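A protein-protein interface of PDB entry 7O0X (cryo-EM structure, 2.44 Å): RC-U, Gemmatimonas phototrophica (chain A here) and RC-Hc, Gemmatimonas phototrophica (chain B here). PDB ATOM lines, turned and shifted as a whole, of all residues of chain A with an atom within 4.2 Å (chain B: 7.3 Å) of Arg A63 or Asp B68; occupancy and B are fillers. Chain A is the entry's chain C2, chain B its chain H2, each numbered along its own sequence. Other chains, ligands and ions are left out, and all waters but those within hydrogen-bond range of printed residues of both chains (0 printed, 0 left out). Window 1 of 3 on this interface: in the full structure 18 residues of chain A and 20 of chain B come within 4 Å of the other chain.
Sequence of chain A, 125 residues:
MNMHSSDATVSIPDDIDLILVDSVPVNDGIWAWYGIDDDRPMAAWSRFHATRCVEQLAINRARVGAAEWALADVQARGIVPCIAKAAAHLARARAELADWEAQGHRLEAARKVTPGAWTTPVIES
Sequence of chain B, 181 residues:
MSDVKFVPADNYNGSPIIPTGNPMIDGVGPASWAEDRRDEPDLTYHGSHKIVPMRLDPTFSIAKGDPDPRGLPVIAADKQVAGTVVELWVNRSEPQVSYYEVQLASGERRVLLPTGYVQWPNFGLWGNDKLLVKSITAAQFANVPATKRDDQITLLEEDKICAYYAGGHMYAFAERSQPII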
ATOM      1  N   ILE A  59       4.467   0.322   2.950  1.00  0.00           N
ATOM      2  CA  ILE A  59       5.152   1.074   1.900  1.00  0.00           C
ATOM      3  C   ILE A  59       4.243   2.129   1.276  1.00  0.00           C
ATOM      4  O   ILE A  59       4.660   3.273   1.065  1.00  0.00           O
ATOM      5  CB  ILE A  59       5.703   0.102   0.839  1.00  0.00           C
ATOM      6  CG1 ILE A  59       6.890  -0.679   1.404  1.00  0.00           C
ATOM      7  CG2 ILE A  59       6.096   0.843  -0.427  1.00  0.00           C
ATOM      8  CD1 ILE A  59       7.250  -1.903   0.600  1.00  0.00           C
ATOM      9  N   ASN A  60       2.992   1.775   0.980  1.00  0.00           N
ATOM     10  CA  ASN A  60       2.091   2.733   0.340  1.00  0.00           C
ATOM     11  C   ASN A  60       1.615   3.841   1.274  1.00  0.00           C
ATOM     12  O   ASN A  60       1.394   4.968   0.817  1.00  0.00           O
ATOM     13  CB  ASN A  60       0.899   1.998  -0.272  1.00  0.00           C
ATOM     14  CG  ASN A  60       1.250   1.328  -1.582  1.00  0.00           C
ATOM     15  OD1 ASN A  60       1.321   1.981  -2.621  1.00  0.00           O
ATOM     16  ND2 ASN A  60       1.491   0.026  -1.539  1.00  0.00           N
ATOM     17  N   ARG A  61       1.445   3.564   2.567  1.00  0.00           N
ATOM     18  CA  ARG A  61       1.147   4.649   3.500  1.00  0.00           C
ATOM     19  C   ARG A  61       2.312   5.624   3.632  1.00  0.00           C
ATOM     20  O   ARG A  61       2.102   6.842   3.684  1.00  0.00           O
ATOM     21  CB  ARG A  61       0.745   4.084   4.860  1.00  0.00           C
ATOM     22  CG  ARG A  61      -0.666   3.527   4.857  1.00  0.00           C
ATOM     23  CD  ARG A  61      -1.179   3.247   6.252  1.00  0.00           C
ATOM     24  NE  ARG A  61      -0.576   2.053   6.825  1.00  0.00           N
ATOM     25  CZ  ARG A  61      -1.262   0.991   7.221  1.00  0.00           C
ATOM     26  NH1 ARG A  61      -2.579   0.938   7.108  1.00  0.00           N
ATOM     27  NH2 ARG A  61      -0.610  -0.047   7.738  1.00  0.00           N
ATOM     28  N   ALA A  62       3.542   5.116   3.692  1.00  0.00           N
ATOM     29  CA  ALA A  62       4.706   5.995   3.631  1.00  0.00           C
ATOM     30  C   ALA A  62       4.748   6.778   2.322  1.00  0.00           C
ATOM     31  O   ALA A  62       5.107   7.960   2.306  1.00  0.00           O
ATOM     32  CB  ALA A  62       5.987   5.179   3.805  1.00  0.00           C
ATOM     33  N   ARG A  63       4.388   6.129   1.216  1.00  0.00           N
ATOM     34  CA  ARG A  63       4.389   6.782  -0.091  1.00  0.00           C
ATOM     35  C   ARG A  63       3.304   7.852  -0.209  1.00  0.00           C
ATOM     36  O   ARG A  63       3.519   8.885  -0.855  1.00  0.00           O
ATOM     37  CB  ARG A  63       4.237   5.721  -1.180  1.00  0.00           C
ATOM     38  CG  ARG A  63       4.501   6.202  -2.589  1.00  0.00           C
ATOM     39  CD  ARG A  63       4.389   5.048  -3.572  1.00  0.00           C
ATOM     40  NE  ARG A  63       5.499   4.114  -3.423  1.00  0.00           N
ATOM     41  CZ  ARG A  63       5.438   2.816  -3.687  1.00  0.00           C
ATOM     42  NH1 ARG A  63       4.284   2.210  -3.912  1.00  0.00           N
ATOM     43  NH2 ARG A  63       6.555   2.097  -3.669  1.00  0.00           N
ATOM     44  N   VAL A  64       2.137   7.628   0.396  1.00  0.00           N
ATOM     45  CA  VAL A  64       1.124   8.681   0.483  1.00  0.00           C
ATOM     46  C   VAL A  64       1.598   9.834   1.360  1.00  0.00           C
ATOM     47  O   VAL A  64       1.402  11.008   1.022  1.00  0.00           O
ATOM     48  CB  VAL A  64      -0.208   8.093   0.986  1.00  0.00           C
ATOM     49  CG1 VAL A  64      -1.142   9.197   1.456  1.00  0.00           C
ATOM     50  CG2 VAL A  64      -0.869   7.288  -0.113  1.00  0.00           C
ATOM     51  N   GLY A  65       2.228   9.524   2.494  1.00  0.00           N
ATOM     52  CA  GLY A  65       2.784  10.571   3.340  1.00  0.00           C
ATOM     53  C   GLY A  65       3.801  11.444   2.630  1.00  0.00           C
ATOM     54  O   GLY A  65       3.760  12.673   2.728  1.00  0.00           O
ATOM     55  N   ALA A  66       4.734  10.822   1.910  1.00  0.00           N
ATOM     56  CA  ALA A  66       5.709  11.581   1.133  1.00  0.00           C
ATOM     57  C   ALA A  66       5.051  12.399   0.026  1.00  0.00           C
ATOM     58  O   ALA A  66       5.465  13.531  -0.243  1.00  0.00           O
ATOM     59  CB  ALA A  66       6.756  10.637   0.545  1.00  0.00           C
ATOM     60  N   ALA A  67       4.031  11.843  -0.631  1.00  0.00           N
ATOM     61  CA  ALA A  67       3.369  12.565  -1.715  1.00  0.00           C
ATOM     62  C   ALA A  67       2.679  13.836  -1.228  1.00  0.00           C
ATOM     63  O   ALA A  67       2.727  14.870  -1.903  1.00  0.00           O
ATOM     64  CB  ALA A  67       2.362  11.647  -2.410  1.00  0.00           C
ATOM     65  N   MET B  54      12.755  15.926  -8.257  1.00  0.00           N
ATOM     66  CA  MET B  54      11.794  15.644  -9.320  1.00  0.00           C
ATOM     67  C   MET B  54      10.477  16.378  -9.096  1.00  0.00           C
ATOM     68  O   MET B  54       9.762  16.692 -10.055  1.00  0.00           O
ATOM     69  CB  MET B  54      11.561  14.136  -9.411  1.00  0.00           C
ATOM     70  CG  MET B  54      10.831  13.684 -10.658  1.00  0.00           C
ATOM     71  SD  MET B  54      10.861  11.894 -10.870  1.00  0.00           S
ATOM     72  CE  MET B  54       9.747  11.383  -9.567  1.00  0.00           C
ATOM     73  N   ILE B  62       8.701   8.236 -12.909  1.00  0.00           N
ATOM     74  CA  ILE B  62       9.189   6.861 -12.968  1.00  0.00           C
ATOM     75  C   ILE B  62       8.605   6.130 -14.173  1.00  0.00           C
ATOM     76  O   ILE B  62       7.418   6.269 -14.496  1.00  0.00           O
ATOM     77  CB  ILE B  62       8.850   6.131 -11.657  1.00  0.00           C
ATOM     78  CG1 ILE B  62       9.565   6.792 -10.481  1.00  0.00           C
ATOM     79  CG2 ILE B  62       9.237   4.662 -11.730  1.00  0.00           C
ATOM     80  CD1 ILE B  62      11.058   6.862 -10.664  1.00  0.00           C
ATOM     81  N   ALA B  63       9.445   5.341 -14.843  1.00  0.00           N
ATOM     82  CA  ALA B  63       9.009   4.550 -15.987  1.00  0.00           C
ATOM     83  C   ALA B  63       8.109   3.390 -15.561  1.00  0.00           C
ATOM     84  O   ALA B  63       8.248   2.831 -14.471  1.00  0.00           O
ATOM     85  CB  ALA B  63      10.220   4.013 -16.750  1.00  0.00           C
ATOM     86  N   GLY B  65       6.847  -0.251 -15.130  1.00  0.00           N
ATOM     87  CA  GLY B  65       7.526  -1.501 -14.857  1.00  0.00           C
ATOM     88  C   GLY B  65       8.697  -1.436 -13.898  1.00  0.00           C
ATOM     89  O   GLY B  65       9.196  -2.494 -13.489  1.00  0.00           O
ATOM     90  N   ASP B  66       9.159  -0.245 -13.524  1.00  0.00           N
ATOM     91  CA  ASP B  66      10.133  -0.136 -12.448  1.00  0.00           C
ATOM     92  C   ASP B  66       9.455   0.157 -11.112  1.00  0.00           C
ATOM     93  O   ASP B  66       8.407   0.807 -11.069  1.00  0.00           O
ATOM     94  CB  ASP B  66      11.156   0.962 -12.755  1.00  0.00           C
ATOM     95  CG  ASP B  66      12.127   0.563 -13.851  1.00  0.00           C
ATOM     96  OD1 ASP B  66      12.227  -0.645 -14.150  1.00  0.00           O
ATOM     97  OD2 ASP B  66      12.795   1.457 -14.410  1.00  0.00           O
ATOM     98  N   PRO B  67      10.025  -0.327 -10.006  1.00  0.00           N
ATOM     99  CA  PRO B  67       9.506   0.047  -8.687  1.00  0.00           C
ATOM    100  C   PRO B  67       9.634   1.545  -8.455  1.00  0.00           C
ATOM    101  O   PRO B  67      10.583   2.185  -8.912  1.00  0.00           O
ATOM    102  CB  PRO B  67      10.386  -0.752  -7.718  1.00  0.00           C
ATOM    103  CG  PRO B  67      11.665  -0.933  -8.451  1.00  0.00           C
ATOM    104  CD  PRO B  67      11.271  -1.105  -9.900  1.00  0.00           C
ATOM    105  N   ASP B  68       8.661   2.109  -7.740  1.00  0.00           N
ATOM    106  CA  ASP B  68       8.781   3.478  -7.259  1.00  0.00           C
ATOM    107  C   ASP B  68       9.547   3.461  -5.941  1.00  0.00           C
ATOM    108  O   ASP B  68       9.041   2.909  -4.952  1.00  0.00           O
ATOM    109  CB  ASP B  68       7.403   4.105  -7.080  1.00  0.00           C
ATOM    110  CG  ASP B  68       7.460   5.589  -6.736  1.00  0.00           C
ATOM    111  OD1 ASP B  68       8.507   6.077  -6.266  1.00  0.00           O
ATOM    112  OD2 ASP B  68       6.441   6.276  -6.951  1.00  0.00           O
ATOM    113  N   PRO B  69      10.750   4.038  -5.876  1.00  0.00           N
ATOM    114  CA  PRO B  69      11.552   3.948  -4.646  1.00  0.00           C
ATOM    115  C   PRO B  69      10.995   4.735  -3.474  1.00  0.00           C
ATOM    116  O   PRO B  69      11.386   4.465  -2.333  1.00  0.00           O
ATOM    117  CB  PRO B  69      12.920   4.500  -5.081  1.00  0.00           C
ATOM    118  CG  PRO B  69      12.922   4.346  -6.576  1.00  0.00           C
ATOM    119  CD  PRO B  69      11.511   4.687  -6.949  1.00  0.00           C
ATOM    120  N   ARG B  70      10.116   5.703  -3.711  1.00  0.00           N
ATOM    121  CA  ARG B  70       9.570   6.504  -2.625  1.00  0.00           C
ATOM    122  C   ARG B  70       8.709   5.658  -1.695  1.00  0.00           C
ATOM    123  O   ARG B  70       7.938   4.803  -2.139  1.00  0.00           O
ATOM    124  CB  ARG B  70       8.760   7.664  -3.199  1.00  0.00           C
ATOM    125  CG  ARG B  70       9.614   8.675  -3.943  1.00  0.00           C
ATOM    126  CD  ARG B  70       8.777   9.666  -4.724  1.00  0.00           C
ATOM    127  NE  ARG B  70       8.163   9.029  -5.883  1.00  0.00           N
ATOM    128  CZ  ARG B  70       7.529   9.676  -6.849  1.00  0.00           C
ATOM    129  NH1 ARG B  70       7.424  10.995  -6.846  1.00  0.00           N
ATOM    130  NH2 ARG B  70       6.997   8.985  -7.853  1.00  0.00           N
ATOM    131  N   GLY B  71       8.844   5.910  -0.393  1.00  0.00           N
ATOM    132  CA  GLY B  71       8.219   5.098   0.631  1.00  0.00           C
ATOM    133  C   GLY B  71       8.950   3.831   1.023  1.00  0.00           C
ATOM    134  O   GLY B  71       8.552   3.192   2.005  1.00  0.00           O
ATOM    135  N   LEU B  72      10.003   3.436   0.303  1.00  0.00           N
ATOM    136  CA  LEU B  72      10.767   2.259   0.710  1.00  0.00           C
ATOM    137  C   LEU B  72      11.663   2.565   1.911  1.00  0.00           C
ATOM    138  O   LEU B  72      12.224   3.657   2.010  1.00  0.00           O
ATOM    139  CB  LEU B  72      11.615   1.740  -0.446  1.00  0.00           C
ATOM    140  CG  LEU B  72      10.861   1.291  -1.697  1.00  0.00           C
ATOM    141  CD1 LEU B  72      11.801   0.580  -2.646  1.00  0.00           C
ATOM    142  CD2 LEU B  72       9.706   0.383  -1.325  1.00  0.00           C
ATOM    143  N   THR B  84      13.405   6.493   5.419  1.00  0.00           N
ATOM    144  CA  THR B  84      12.524   6.225   4.290  1.00  0.00           C
ATOM    145  C   THR B  84      12.854   7.176   3.147  1.00  0.00           C
ATOM    146  O   THR B  84      13.104   8.362   3.374  1.00  0.00           O
ATOM    147  CB  THR B  84      11.054   6.381   4.712  1.00  0.00           C
ATOM    148  OG1 THR B  84      10.698   5.320   5.606  1.00  0.00           O
ATOM    149  CG2 THR B  84      10.127   6.345   3.508  1.00  0.00           C
ATOM    150  N   VAL B  85      12.854   6.658   1.917  1.00  0.00           N
ATOM    151  CA  VAL B  85      12.980   7.526   0.751  1.00  0.00           C
ATOM    152  C   VAL B  85      11.714   8.356   0.601  1.00  0.00           C
ATOM    153  O   VAL B  85      10.600   7.821   0.571  1.00  0.00           O
ATOM    154  CB  VAL B  85      13.254   6.701  -0.513  1.00  0.00           C
ATOM    155  CG1 VAL B  85      13.322   7.607  -1.732  1.00  0.00           C
ATOM    156  CG2 VAL B  85      14.542   5.923  -0.363  1.00  0.00           C
ATOM    157  N   VAL B  86      11.881   9.672   0.502  1.00  0.00           N
ATOM    158  CA  VAL B  86      10.751  10.573   0.321  1.00  0.00           C
ATOM    159  C   VAL B  86      10.812  11.361  -0.979  1.00  0.00           C
ATOM    160  O   VAL B  86       9.786  11.933  -1.383  1.00  0.00           O
ATOM    161  CB  VAL B  86      10.612  11.539   1.516  1.00  0.00           C
ATOM    162  CG1 VAL B  86      10.266  10.772   2.778  1.00  0.00           C
ATOM    163  CG2 VAL B  86      11.888  12.338   1.702  1.00  0.00           C
ATOM    164  N   LEU B  88      13.080  11.938  -5.055  1.00  0.00           N
ATOM    165  CA  LEU B  88      14.104  11.621  -6.042  1.00  0.00           C
ATOM    166  C   LEU B  88      14.687  12.909  -6.609  1.00  0.00           C
ATOM    167  O   LEU B  88      13.958  13.877  -6.837  1.00  0.00           O
ATOM    168  CB  LEU B  88      13.516  10.788  -7.180  1.00  0.00           C
ATOM    169  CG  LEU B  88      12.624   9.608  -6.795  1.00  0.00           C
ATOM    170  CD1 LEU B  88      12.211   8.857  -8.034  1.00  0.00           C
ATOM    171  CD2 LEU B  88      13.322   8.679  -5.827  1.00  0.00           C
ATOM    172  N   TYR B 100      18.681   9.584  -4.106  1.00  0.00           N
ATOM    173  CA  TYR B 100      17.515   9.426  -3.257  1.00  0.00           C
ATOM    174  C   TYR B 100      17.644  10.394  -2.091  1.00  0.00           C
ATOM    175  O   TYR B 100      18.732  10.573  -1.539  1.00  0.00           O
ATOM    176  CB  TYR B 100      17.411   7.989  -2.751  1.00  0.00           C
ATOM    177  CG  TYR B 100      17.233   6.982  -3.860  1.00  0.00           C
ATOM    178  CD1 TYR B 100      16.146   7.049  -4.713  1.00  0.00           C
ATOM    179  CD2 TYR B 100      18.162   5.973  -4.063  1.00  0.00           C
ATOM    180  CE1 TYR B 100      15.988   6.145  -5.741  1.00  0.00           C
ATOM    181  CE2 TYR B 100      18.007   5.055  -5.082  1.00  0.00           C
ATOM    182  CZ  TYR B 100      16.918   5.148  -5.919  1.00  0.00           C
ATOM    183  OH  TYR B 100      16.748   4.231  -6.929  1.00  0.00           O
ATOM    184  N   TRP B 120      19.606  -3.025  -4.648  1.00  0.00           N
ATOM    185  CA  TRP B 120      18.303  -3.655  -4.504  1.00  0.00           C
ATOM    186  C   TRP B 120      18.444  -5.108  -4.039  1.00  0.00           C
ATOM    187  O   TRP B 120      19.465  -5.749  -4.296  1.00  0.00           O
ATOM    188  CB  TRP B 120      17.546  -3.576  -5.824  1.00  0.00           C
ATOM    189  CG  TRP B 120      17.171  -2.161  -6.162  1.00  0.00           C
ATOM    190  CD1 TRP B 120      17.959  -1.234  -6.778  1.00  0.00           C
ATOM    191  CD2 TRP B 120      15.926  -1.506  -5.886  1.00  0.00           C
ATOM    192  NE1 TRP B 120      17.283  -0.048  -6.909  1.00  0.00           N
ATOM    193  CE2 TRP B 120      16.031  -0.188  -6.371  1.00  0.00           C
ATOM    194  CE3 TRP B 120      14.732  -1.908  -5.281  1.00  0.00           C
ATOM    195  CZ2 TRP B 120      14.988   0.731  -6.270  1.00  0.00           C
ATOM    196  CZ3 TRP B 120      13.698  -0.995  -5.184  1.00  0.00           C
ATOM    197  CH2 TRP B 120      13.832   0.308  -5.675  1.00  0.00           C
ATOM    198  N   ASN B 128      12.236  -6.117  -4.273  1.00  0.00           N
ATOM    199  CA  ASN B 128      12.141  -4.704  -4.650  1.00  0.00           C
ATOM    200  C   ASN B 128      11.341  -3.869  -3.650  1.00  0.00           C
ATOM    201  O   ASN B 128      10.573  -2.980  -4.022  1.00  0.00           O
ATOM    202  CB  ASN B 128      11.584  -4.565  -6.065  1.00  0.00           C
ATOM    203  CG  ASN B 128      12.494  -5.197  -7.103  1.00  0.00           C
ATOM    204  OD1 ASN B 128      13.713  -5.038  -7.049  1.00  0.00           O
ATOM    205  ND2 ASN B 128      11.909  -5.921  -8.046  1.00  0.00           N
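The guanidinium group (NE) of Arg A63 is in hydrogen-bond range of the backbone carbonyl oxygen (O) of Arg B70, 2.8 Å away.
The guanidinium group (NH2) of Arg A63 is in hydrogen-bond range of the backbone carbonyl oxygen (O) of Asp B68.
The guanidinium group (NH1) of Arg A63 lies within hydrogen-bond range of the side-chain amide oxygen (OD1) of Asn A60, 3.2 Å away.
The side-chain carboxylate (OD2) of Asp B68 lies within salt-bridge range of the guanidinium group (NH2) of Arg B70.
N of Gly B71 is in hydrogen-bond range of O of Val B85 (2.8 Å).
The backbone carbonyl oxygen (O) of Leu B72 sits at hydrogen-bond distance from the backbone NH (N) of Val B85, at 3.1 Å.
Ile A59 touches Leu B72 (CG2 to CD2, 3.7 Å).
Ala A62 touches Gly B71.
CB of Ala A66 touches O of Val B86, at 3.8 Å.
Of the printed residues of chain B, Arg A63 touches Asp B68 (2.9 Å) and Arg B70 (2.8 Å).
Asp B68 touches just one residue of chain A: Arg A63 (2.9 Å).
Of chain B, only Gly B71 (3.7 Å) comes within 4 Å of Ala A62.
Of the printed residues of chain B, Ile A59 touches Leu B72 (3.7 Å).
Printed residues of chain B within 4 Å of Ala A66: Val B86 (3.8 Å).
Printed residues of chain A within 4 Å of Val B86: Ala A66.
Of the printed residues of chain A, Leu B72 touches Ile A59.
Ala A67 touches none of the printed residues of chain B.
Of the 18 printed residues of chain B, 5 touch a printed residue of chain A.
Printed residues of chain B that touch a printed residue of chain A: Asp B68, Arg B70, Gly B71, Leu B72 and Val B86.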
